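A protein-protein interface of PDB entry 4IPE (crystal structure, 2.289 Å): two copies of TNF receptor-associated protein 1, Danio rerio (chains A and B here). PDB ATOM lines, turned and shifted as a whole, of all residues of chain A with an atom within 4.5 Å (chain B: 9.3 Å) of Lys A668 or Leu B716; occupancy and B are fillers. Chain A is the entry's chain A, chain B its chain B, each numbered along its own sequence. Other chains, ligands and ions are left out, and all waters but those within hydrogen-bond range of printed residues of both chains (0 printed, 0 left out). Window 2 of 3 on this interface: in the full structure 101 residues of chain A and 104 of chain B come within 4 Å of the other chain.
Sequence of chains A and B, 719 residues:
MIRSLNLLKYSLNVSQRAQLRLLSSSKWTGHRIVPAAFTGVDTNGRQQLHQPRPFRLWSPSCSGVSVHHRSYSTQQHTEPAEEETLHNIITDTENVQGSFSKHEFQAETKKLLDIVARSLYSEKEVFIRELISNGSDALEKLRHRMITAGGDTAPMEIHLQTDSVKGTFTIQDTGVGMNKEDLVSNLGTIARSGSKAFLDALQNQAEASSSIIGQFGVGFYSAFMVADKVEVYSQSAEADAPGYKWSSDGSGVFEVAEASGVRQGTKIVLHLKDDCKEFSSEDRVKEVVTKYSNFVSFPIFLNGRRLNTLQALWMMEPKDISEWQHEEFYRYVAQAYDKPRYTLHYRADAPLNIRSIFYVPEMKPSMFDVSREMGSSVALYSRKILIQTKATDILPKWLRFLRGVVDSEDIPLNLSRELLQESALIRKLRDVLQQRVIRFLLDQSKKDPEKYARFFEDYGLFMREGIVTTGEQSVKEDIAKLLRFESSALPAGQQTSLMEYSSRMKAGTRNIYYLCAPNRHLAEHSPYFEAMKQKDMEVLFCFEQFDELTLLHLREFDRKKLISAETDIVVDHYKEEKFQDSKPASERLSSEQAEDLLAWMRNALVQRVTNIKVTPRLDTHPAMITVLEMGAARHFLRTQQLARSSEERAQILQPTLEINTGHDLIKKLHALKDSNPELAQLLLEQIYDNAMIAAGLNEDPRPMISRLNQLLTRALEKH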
ATOM      1  N   ASP A 664     -12.223  -4.676  31.888  1.00  0.00           N
ATOM      2  CA  ASP A 664     -13.663  -4.449  31.799  1.00  0.00           C
ATOM      3  C   ASP A 664     -14.391  -5.516  30.997  1.00  0.00           C
ATOM      4  O   ASP A 664     -15.485  -5.930  31.368  1.00  0.00           O
ATOM      5  CB  ASP A 664     -13.956  -3.072  31.206  1.00  0.00           C
ATOM      6  CG  ASP A 664     -13.344  -1.950  32.019  1.00  0.00           C
ATOM      7  OD1 ASP A 664     -13.247  -2.086  33.264  1.00  0.00           O
ATOM      8  OD2 ASP A 664     -12.961  -0.929  31.413  1.00  0.00           O
ATOM      9  N   LEU A 665     -13.786  -5.954  29.900  1.00  0.00           N
ATOM     10  CA  LEU A 665     -14.391  -6.987  29.069  1.00  0.00           C
ATOM     11  C   LEU A 665     -14.489  -8.323  29.800  1.00  0.00           C
ATOM     12  O   LEU A 665     -15.439  -9.077  29.596  1.00  0.00           O
ATOM     13  CB  LEU A 665     -13.602  -7.169  27.780  1.00  0.00           C
ATOM     14  CG  LEU A 665     -13.678  -6.002  26.798  1.00  0.00           C
ATOM     15  CD1 LEU A 665     -12.768  -6.278  25.616  1.00  0.00           C
ATOM     16  CD2 LEU A 665     -15.114  -5.744  26.351  1.00  0.00           C
ATOM     17  N   ILE A 666     -13.500  -8.608  30.642  1.00  0.00           N
ATOM     18  CA  ILE A 666     -13.506  -9.824  31.446  1.00  0.00           C
ATOM     19  C   ILE A 666     -14.593  -9.756  32.506  1.00  0.00           C
ATOM     20  O   ILE A 666     -15.341 -10.717  32.713  1.00  0.00           O
ATOM     21  CB  ILE A 666     -12.157 -10.043  32.136  1.00  0.00           C
ATOM     22  CG1 ILE A 666     -11.100 -10.454  31.105  1.00  0.00           C
ATOM     23  CG2 ILE A 666     -12.284 -11.082  33.259  1.00  0.00           C
ATOM     24  CD1 ILE A 666     -11.419 -11.734  30.365  1.00  0.00           C
ATOM     25  N   LYS A 667     -14.677  -8.616  33.178  1.00  0.00           N
ATOM     26  CA  LYS A 667     -15.724  -8.421  34.166  1.00  0.00           C
ATOM     27  C   LYS A 667     -17.082  -8.425  33.477  1.00  0.00           C
ATOM     28  O   LYS A 667     -18.055  -8.916  34.040  1.00  0.00           O
ATOM     29  CB  LYS A 667     -15.498  -7.137  34.960  1.00  0.00           C
ATOM     30  CG  LYS A 667     -14.234  -7.187  35.805  1.00  0.00           C
ATOM     31  CD  LYS A 667     -14.159  -6.032  36.784  1.00  0.00           C
ATOM     32  CE  LYS A 667     -13.833  -4.727  36.084  1.00  0.00           C
ATOM     33  NZ  LYS A 667     -13.505  -3.681  37.092  1.00  0.00           N
ATOM     34  N   LYS A 668     -17.138  -7.908  32.250  1.00  0.00           N
ATOM     35  CA  LYS A 668     -18.370  -7.963  31.460  1.00  0.00           C
ATOM     36  C   LYS A 668     -18.683  -9.407  31.079  1.00  0.00           C
ATOM     37  O   LYS A 668     -19.841  -9.831  31.126  1.00  0.00           O
ATOM     38  CB  LYS A 668     -18.280  -7.069  30.212  1.00  0.00           C
ATOM     39  CG  LYS A 668     -18.544  -5.580  30.486  1.00  0.00           C
ATOM     40  CD  LYS A 668     -20.032  -5.290  30.730  1.00  0.00           C
ATOM     41  CE  LYS A 668     -20.252  -3.907  31.345  1.00  0.00           C
ATOM     42  NZ  LYS A 668     -19.939  -3.874  32.808  1.00  0.00           N
ATOM     43  N   LEU A 669     -17.638 -10.158  30.731  1.00  0.00           N
ATOM     44  CA  LEU A 669     -17.770 -11.575  30.398  1.00  0.00           C
ATOM     45  C   LEU A 669     -18.325 -12.358  31.573  1.00  0.00           C
ATOM     46  O   LEU A 669     -19.219 -13.195  31.415  1.00  0.00           O
ATOM     47  CB  LEU A 669     -16.415 -12.155  30.015  1.00  0.00           C
ATOM     48  CG  LEU A 669     -16.449 -13.643  29.682  1.00  0.00           C
ATOM     49  CD1 LEU A 669     -17.272 -13.894  28.422  1.00  0.00           C
ATOM     50  CD2 LEU A 669     -15.045 -14.202  29.543  1.00  0.00           C
ATOM     51  N   HIS A 670     -17.779 -12.079  32.751  1.00  0.00           N
ATOM     52  CA  HIS A 670     -18.247 -12.690  33.984  1.00  0.00           C
ATOM     53  C   HIS A 670     -19.752 -12.492  34.174  1.00  0.00           C
ATOM     54  O   HIS A 670     -20.464 -13.425  34.546  1.00  0.00           O
ATOM     55  CB  HIS A 670     -17.479 -12.111  35.178  1.00  0.00           C
ATOM     56  CG  HIS A 670     -18.051 -12.500  36.506  1.00  0.00           C
ATOM     57  ND1 HIS A 670     -18.771 -11.622  37.289  1.00  0.00           N
ATOM     58  CD2 HIS A 670     -18.022 -13.672  37.181  1.00  0.00           C
ATOM     59  CE1 HIS A 670     -19.156 -12.237  38.396  1.00  0.00           C
ATOM     60  NE2 HIS A 670     -18.716 -13.484  38.353  1.00  0.00           N
ATOM     61  N   ALA A 671     -20.229 -11.281  33.897  1.00  0.00           N
ATOM     62  CA  ALA A 671     -21.627 -10.934  34.141  1.00  0.00           C
ATOM     63  C   ALA A 671     -22.562 -11.542  33.102  1.00  0.00           C
ATOM     64  O   ALA A 671     -23.695 -11.900  33.413  1.00  0.00           O
ATOM     65  CB  ALA A 671     -21.799  -9.415  34.190  1.00  0.00           C
ATOM     66  N   LEU A 672     -22.078 -11.671  31.872  1.00  0.00           N
ATOM     67  CA  LEU A 672     -22.937 -12.111  30.782  1.00  0.00           C
ATOM     68  C   LEU A 672     -23.035 -13.623  30.634  1.00  0.00           C
ATOM     69  O   LEU A 672     -23.902 -14.110  29.919  1.00  0.00           O
ATOM     70  CB  LEU A 672     -22.459 -11.515  29.466  1.00  0.00           C
ATOM     71  CG  LEU A 672     -22.399  -9.995  29.376  1.00  0.00           C
ATOM     72  CD1 LEU A 672     -21.458  -9.614  28.251  1.00  0.00           C
ATOM     73  CD2 LEU A 672     -23.778  -9.409  29.149  1.00  0.00           C
ATOM     74  N   LEU A 683     -18.377 -13.142  22.834  1.00  0.00           N
ATOM     75  CA  LEU A 683     -17.379 -12.279  23.444  1.00  0.00           C
ATOM     76  C   LEU A 683     -16.160 -13.097  23.813  1.00  0.00           C
ATOM     77  O   LEU A 683     -15.025 -12.688  23.552  1.00  0.00           O
ATOM     78  CB  LEU A 683     -17.924 -11.559  24.675  1.00  0.00           C
ATOM     79  CG  LEU A 683     -16.871 -10.810  25.512  1.00  0.00           C
ATOM     80  CD1 LEU A 683     -16.001  -9.829  24.684  1.00  0.00           C
ATOM     81  CD2 LEU A 683     -17.517 -10.086  26.685  1.00  0.00           C
ATOM     82  N   ALA A 715     -24.385  -6.715  20.292  1.00  0.00           N
ATOM     83  CA  ALA A 715     -23.928  -5.850  21.365  1.00  0.00           C
ATOM     84  C   ALA A 715     -24.578  -4.478  21.249  1.00  0.00           C
ATOM     85  O   ALA A 715     -24.797  -3.803  22.250  1.00  0.00           O
ATOM     86  CB  ALA A 715     -22.408  -5.724  21.342  1.00  0.00           C
ATOM     87  N   LEU B 679     -19.065   6.748  19.125  1.00  0.00           N
ATOM     88  CA  LEU B 679     -19.206   5.303  19.019  1.00  0.00           C
ATOM     89  C   LEU B 679     -19.450   4.909  17.564  1.00  0.00           C
ATOM     90  O   LEU B 679     -18.918   3.900  17.091  1.00  0.00           O
ATOM     91  CB  LEU B 679     -20.344   4.818  19.917  1.00  0.00           C
ATOM     92  CG  LEU B 679     -20.741   3.345  19.830  1.00  0.00           C
ATOM     93  CD1 LEU B 679     -19.557   2.462  20.145  1.00  0.00           C
ATOM     94  CD2 LEU B 679     -21.909   3.071  20.763  1.00  0.00           C
ATOM     95  N   LEU B 708     -10.546  -2.433  18.742  1.00  0.00           N
ATOM     96  CA  LEU B 708     -11.618  -3.416  18.814  1.00  0.00           C
ATOM     97  C   LEU B 708     -12.043  -3.630  20.261  1.00  0.00           C
ATOM     98  O   LEU B 708     -13.233  -3.597  20.564  1.00  0.00           O
ATOM     99  CB  LEU B 708     -11.176  -4.735  18.178  1.00  0.00           C
ATOM    100  CG  LEU B 708     -12.241  -5.836  18.182  1.00  0.00           C
ATOM    101  CD1 LEU B 708     -13.599  -5.343  17.630  1.00  0.00           C
ATOM    102  CD2 LEU B 708     -11.739  -7.066  17.415  1.00  0.00           C
ATOM    103  N   ASN B 709     -11.068  -3.833  21.149  1.00  0.00           N
ATOM    104  CA  ASN B 709     -11.352  -3.959  22.573  1.00  0.00           C
ATOM    105  C   ASN B 709     -12.054  -2.711  23.109  1.00  0.00           C
ATOM    106  O   ASN B 709     -13.041  -2.816  23.835  1.00  0.00           O
ATOM    107  CB  ASN B 709     -10.072  -4.241  23.376  1.00  0.00           C
ATOM    108  CG  ASN B 709      -9.550  -5.658  23.169  1.00  0.00           C
ATOM    109  OD1 ASN B 709     -10.271  -6.531  22.683  1.00  0.00           O
ATOM    110  ND2 ASN B 709      -8.297  -5.894  23.550  1.00  0.00           N
ATOM    111  N   GLN B 710     -11.540  -1.538  22.738  1.00  0.00           N
ATOM    112  CA  GLN B 710     -12.176  -0.268  23.077  1.00  0.00           C
ATOM    113  C   GLN B 710     -13.604  -0.202  22.548  1.00  0.00           C
ATOM    114  O   GLN B 710     -14.524   0.130  23.288  1.00  0.00           O
ATOM    115  CB  GLN B 710     -11.365   0.892  22.517  1.00  0.00           C
ATOM    116  CG  GLN B 710     -10.110   1.197  23.334  1.00  0.00           C
ATOM    117  CD  GLN B 710      -9.169   2.168  22.633  1.00  0.00           C
ATOM    118  OE1 GLN B 710      -9.309   2.437  21.434  1.00  0.00           O
ATOM    119  NE2 GLN B 710      -8.202   2.696  23.380  1.00  0.00           N
ATOM    120  N   LEU B 711     -13.781  -0.527  21.271  1.00  0.00           N
ATOM    121  CA  LEU B 711     -15.112  -0.577  20.689  1.00  0.00           C
ATOM    122  C   LEU B 711     -16.000  -1.554  21.456  1.00  0.00           C
ATOM    123  O   LEU B 711     -17.151  -1.234  21.775  1.00  0.00           O
ATOM    124  CB  LEU B 711     -15.048  -0.979  19.217  1.00  0.00           C
ATOM    125  CG  LEU B 711     -16.419  -1.076  18.536  1.00  0.00           C
ATOM    126  CD1 LEU B 711     -17.209   0.216  18.666  1.00  0.00           C
ATOM    127  CD2 LEU B 711     -16.271  -1.471  17.070  1.00  0.00           C
ATOM    128  N   LEU B 712     -15.455  -2.730  21.768  1.00  0.00           N
ATOM    129  CA  LEU B 712     -16.215  -3.748  22.487  1.00  0.00           C
ATOM    130  C   LEU B 712     -16.705  -3.283  23.855  1.00  0.00           C
ATOM    131  O   LEU B 712     -17.848  -3.554  24.224  1.00  0.00           O
ATOM    132  CB  LEU B 712     -15.415  -5.043  22.607  1.00  0.00           C
ATOM    133  CG  LEU B 712     -15.361  -5.852  21.309  1.00  0.00           C
ATOM    134  CD1 LEU B 712     -14.610  -7.154  21.485  1.00  0.00           C
ATOM    135  CD2 LEU B 712     -16.755  -6.116  20.768  1.00  0.00           C
ATOM    136  N   THR B 713     -15.865  -2.577  24.606  1.00  0.00           N
ATOM    137  CA  THR B 713     -16.291  -2.123  25.926  1.00  0.00           C
ATOM    138  C   THR B 713     -17.385  -1.062  25.813  1.00  0.00           C
ATOM    139  O   THR B 713     -18.375  -1.115  26.536  1.00  0.00           O
ATOM    140  CB  THR B 713     -15.150  -1.528  26.764  1.00  0.00           C
ATOM    141  OG1 THR B 713     -14.865  -0.204  26.304  1.00  0.00           O
ATOM    142  CG2 THR B 713     -13.898  -2.376  26.688  1.00  0.00           C
ATOM    143  N   ARG B 714     -17.211  -0.105  24.900  1.00  0.00           N
ATOM    144  CA  ARG B 714     -18.174   0.991  24.783  1.00  0.00           C
ATOM    145  C   ARG B 714     -19.529   0.497  24.297  1.00  0.00           C
ATOM    146  O   ARG B 714     -20.571   1.058  24.642  1.00  0.00           O
ATOM    147  CB  ARG B 714     -17.664   2.121  23.884  1.00  0.00           C
ATOM    148  CG  ARG B 714     -18.448   3.411  24.109  1.00  0.00           C
ATOM    149  CD  ARG B 714     -17.897   4.580  23.343  1.00  0.00           C
ATOM    150  NE  ARG B 714     -16.448   4.657  23.440  1.00  0.00           N
ATOM    151  CZ  ARG B 714     -15.761   5.782  23.281  1.00  0.00           C
ATOM    152  NH1 ARG B 714     -16.404   6.917  23.038  1.00  0.00           N
ATOM    153  NH2 ARG B 714     -14.436   5.777  23.377  1.00  0.00           N
ATOM    154  N   ALA B 715     -19.503  -0.568  23.508  1.00  0.00           N
ATOM    155  CA  ALA B 715     -20.732  -1.199  23.061  1.00  0.00           C
ATOM    156  C   ALA B 715     -21.426  -1.898  24.227  1.00  0.00           C
ATOM    157  O   ALA B 715     -22.599  -1.644  24.503  1.00  0.00           O
ATOM    158  CB  ALA B 715     -20.438  -2.180  21.950  1.00  0.00           C
ATOM    159  N   LEU B 716     -20.691  -2.761  24.925  1.00  0.00           N
ATOM    160  CA  LEU B 716     -21.260  -3.541  26.025  1.00  0.00           C
ATOM    161  C   LEU B 716     -21.680  -2.737  27.249  1.00  0.00           C
ATOM    162  O   LEU B 716     -21.926  -3.311  28.311  1.00  0.00           O
ATOM    163  CB  LEU B 716     -20.326  -4.690  26.399  1.00  0.00           C
ATOM    164  CG  LEU B 716     -19.967  -5.685  25.300  1.00  0.00           C
ATOM    165  CD1 LEU B 716     -18.993  -6.711  25.859  1.00  0.00           C
ATOM    166  CD2 LEU B 716     -21.213  -6.350  24.734  1.00  0.00           C
ATOM    167  N   GLU B 717     -21.764  -1.416  27.086  1.00  0.00           N
ATOM    168  CA  GLU B 717     -22.146  -0.484  28.150  1.00  0.00           C
ATOM    169  C   GLU B 717     -20.953  -0.288  29.081  1.00  0.00           C
ATOM    170  O   GLU B 717     -20.085   0.549  28.828  1.00  0.00           O
ATOM    171  CB  GLU B 717     -23.383  -0.921  28.944  1.00  0.00           C
ATOM    172  CG  GLU B 717     -24.574  -1.293  28.074  1.00  0.00           C
ATOM    173  CD  GLU B 717     -25.397  -2.417  28.672  1.00  0.00           C
ATOM    174  OE1 GLU B 717     -26.588  -2.529  28.327  1.00  0.00           O
ATOM    175  OE2 GLU B 717     -24.855  -3.196  29.484  1.00  0.00           O
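Ala B715 touches its own counterpart, Ala A715.
Position printed for both chains: 715.
Of the 7 pairs that touch across the chains among the printed residues, 1 has its exchanged pair printed and touching as well.
Of the 11 printed residues of chain A, 4 touch a printed residue of chain B.
Hydrophobic or aromatic side chains of chain A that line the printed part of chain B: Leu A665, Leu A683 and Ala A715.
Of the 11 printed residues of chain B, 5 touch a printed residue of chain A.
Printed residues of chain B that touch a printed residue of chain A: Asn B709, Leu B712, Thr B713, Ala B715 and Leu B716.
Hydrophobic or aromatic side chains of chain B that line the printed part of chain A: Leu B712 and Leu B716.
Among the printed residues, 7 pairs touch across the chains.
Among the printed residues, no Asp or Glu carboxylate lies within 4 Å of a Lys or Arg side-chain nitrogen of the other chain.
The backbone carbonyl oxygen (O) of Gln B710 sits at hydrogen-bond distance from the side-chain hydroxyl (OG1) of Thr B713.
Of chain B, only Leu B716 comes within 4 Å of Lys A668.
No residue of chain B comes within 4 Å of Ala A671.
Printed residues of chain B within 4 Å of Leu A683: Leu B716.
Of the printed residues of chain A, Ala B715 touches Ala A715.
Leu B716 touches just these residues of chain A: Lys A668 (3.5 Å), Leu A683 (3.8 Å) and Ala A715 (3.7 Å).
The nearest residue of chain B that does not touch Lys A668 is Glu B717 (4.3 Å).
The nearest residue of chain A that does not touch Leu B716 is Leu A665 (4.03 Å).
The nearest printed residue of chain B that does not touch Leu A665 is Leu B716 (4.03 Å).
Leu A665 touches Asn B709.
CB of Leu B712 touches CD2 of Leu A665, 3.8 Å away.
CD2 of Leu A665 touches CG2 of Thr B713 (3.6 Å).
Leu B716 touches Lys A668 (O to CE, 3.5 Å).
CD1 of Leu B716 touches CD2 of Leu A683, 3.8 Å away.
Ala B715 touches Ala A715.
CB of Ala A715 touches CD2 of Leu B716, at 3.7 Å.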
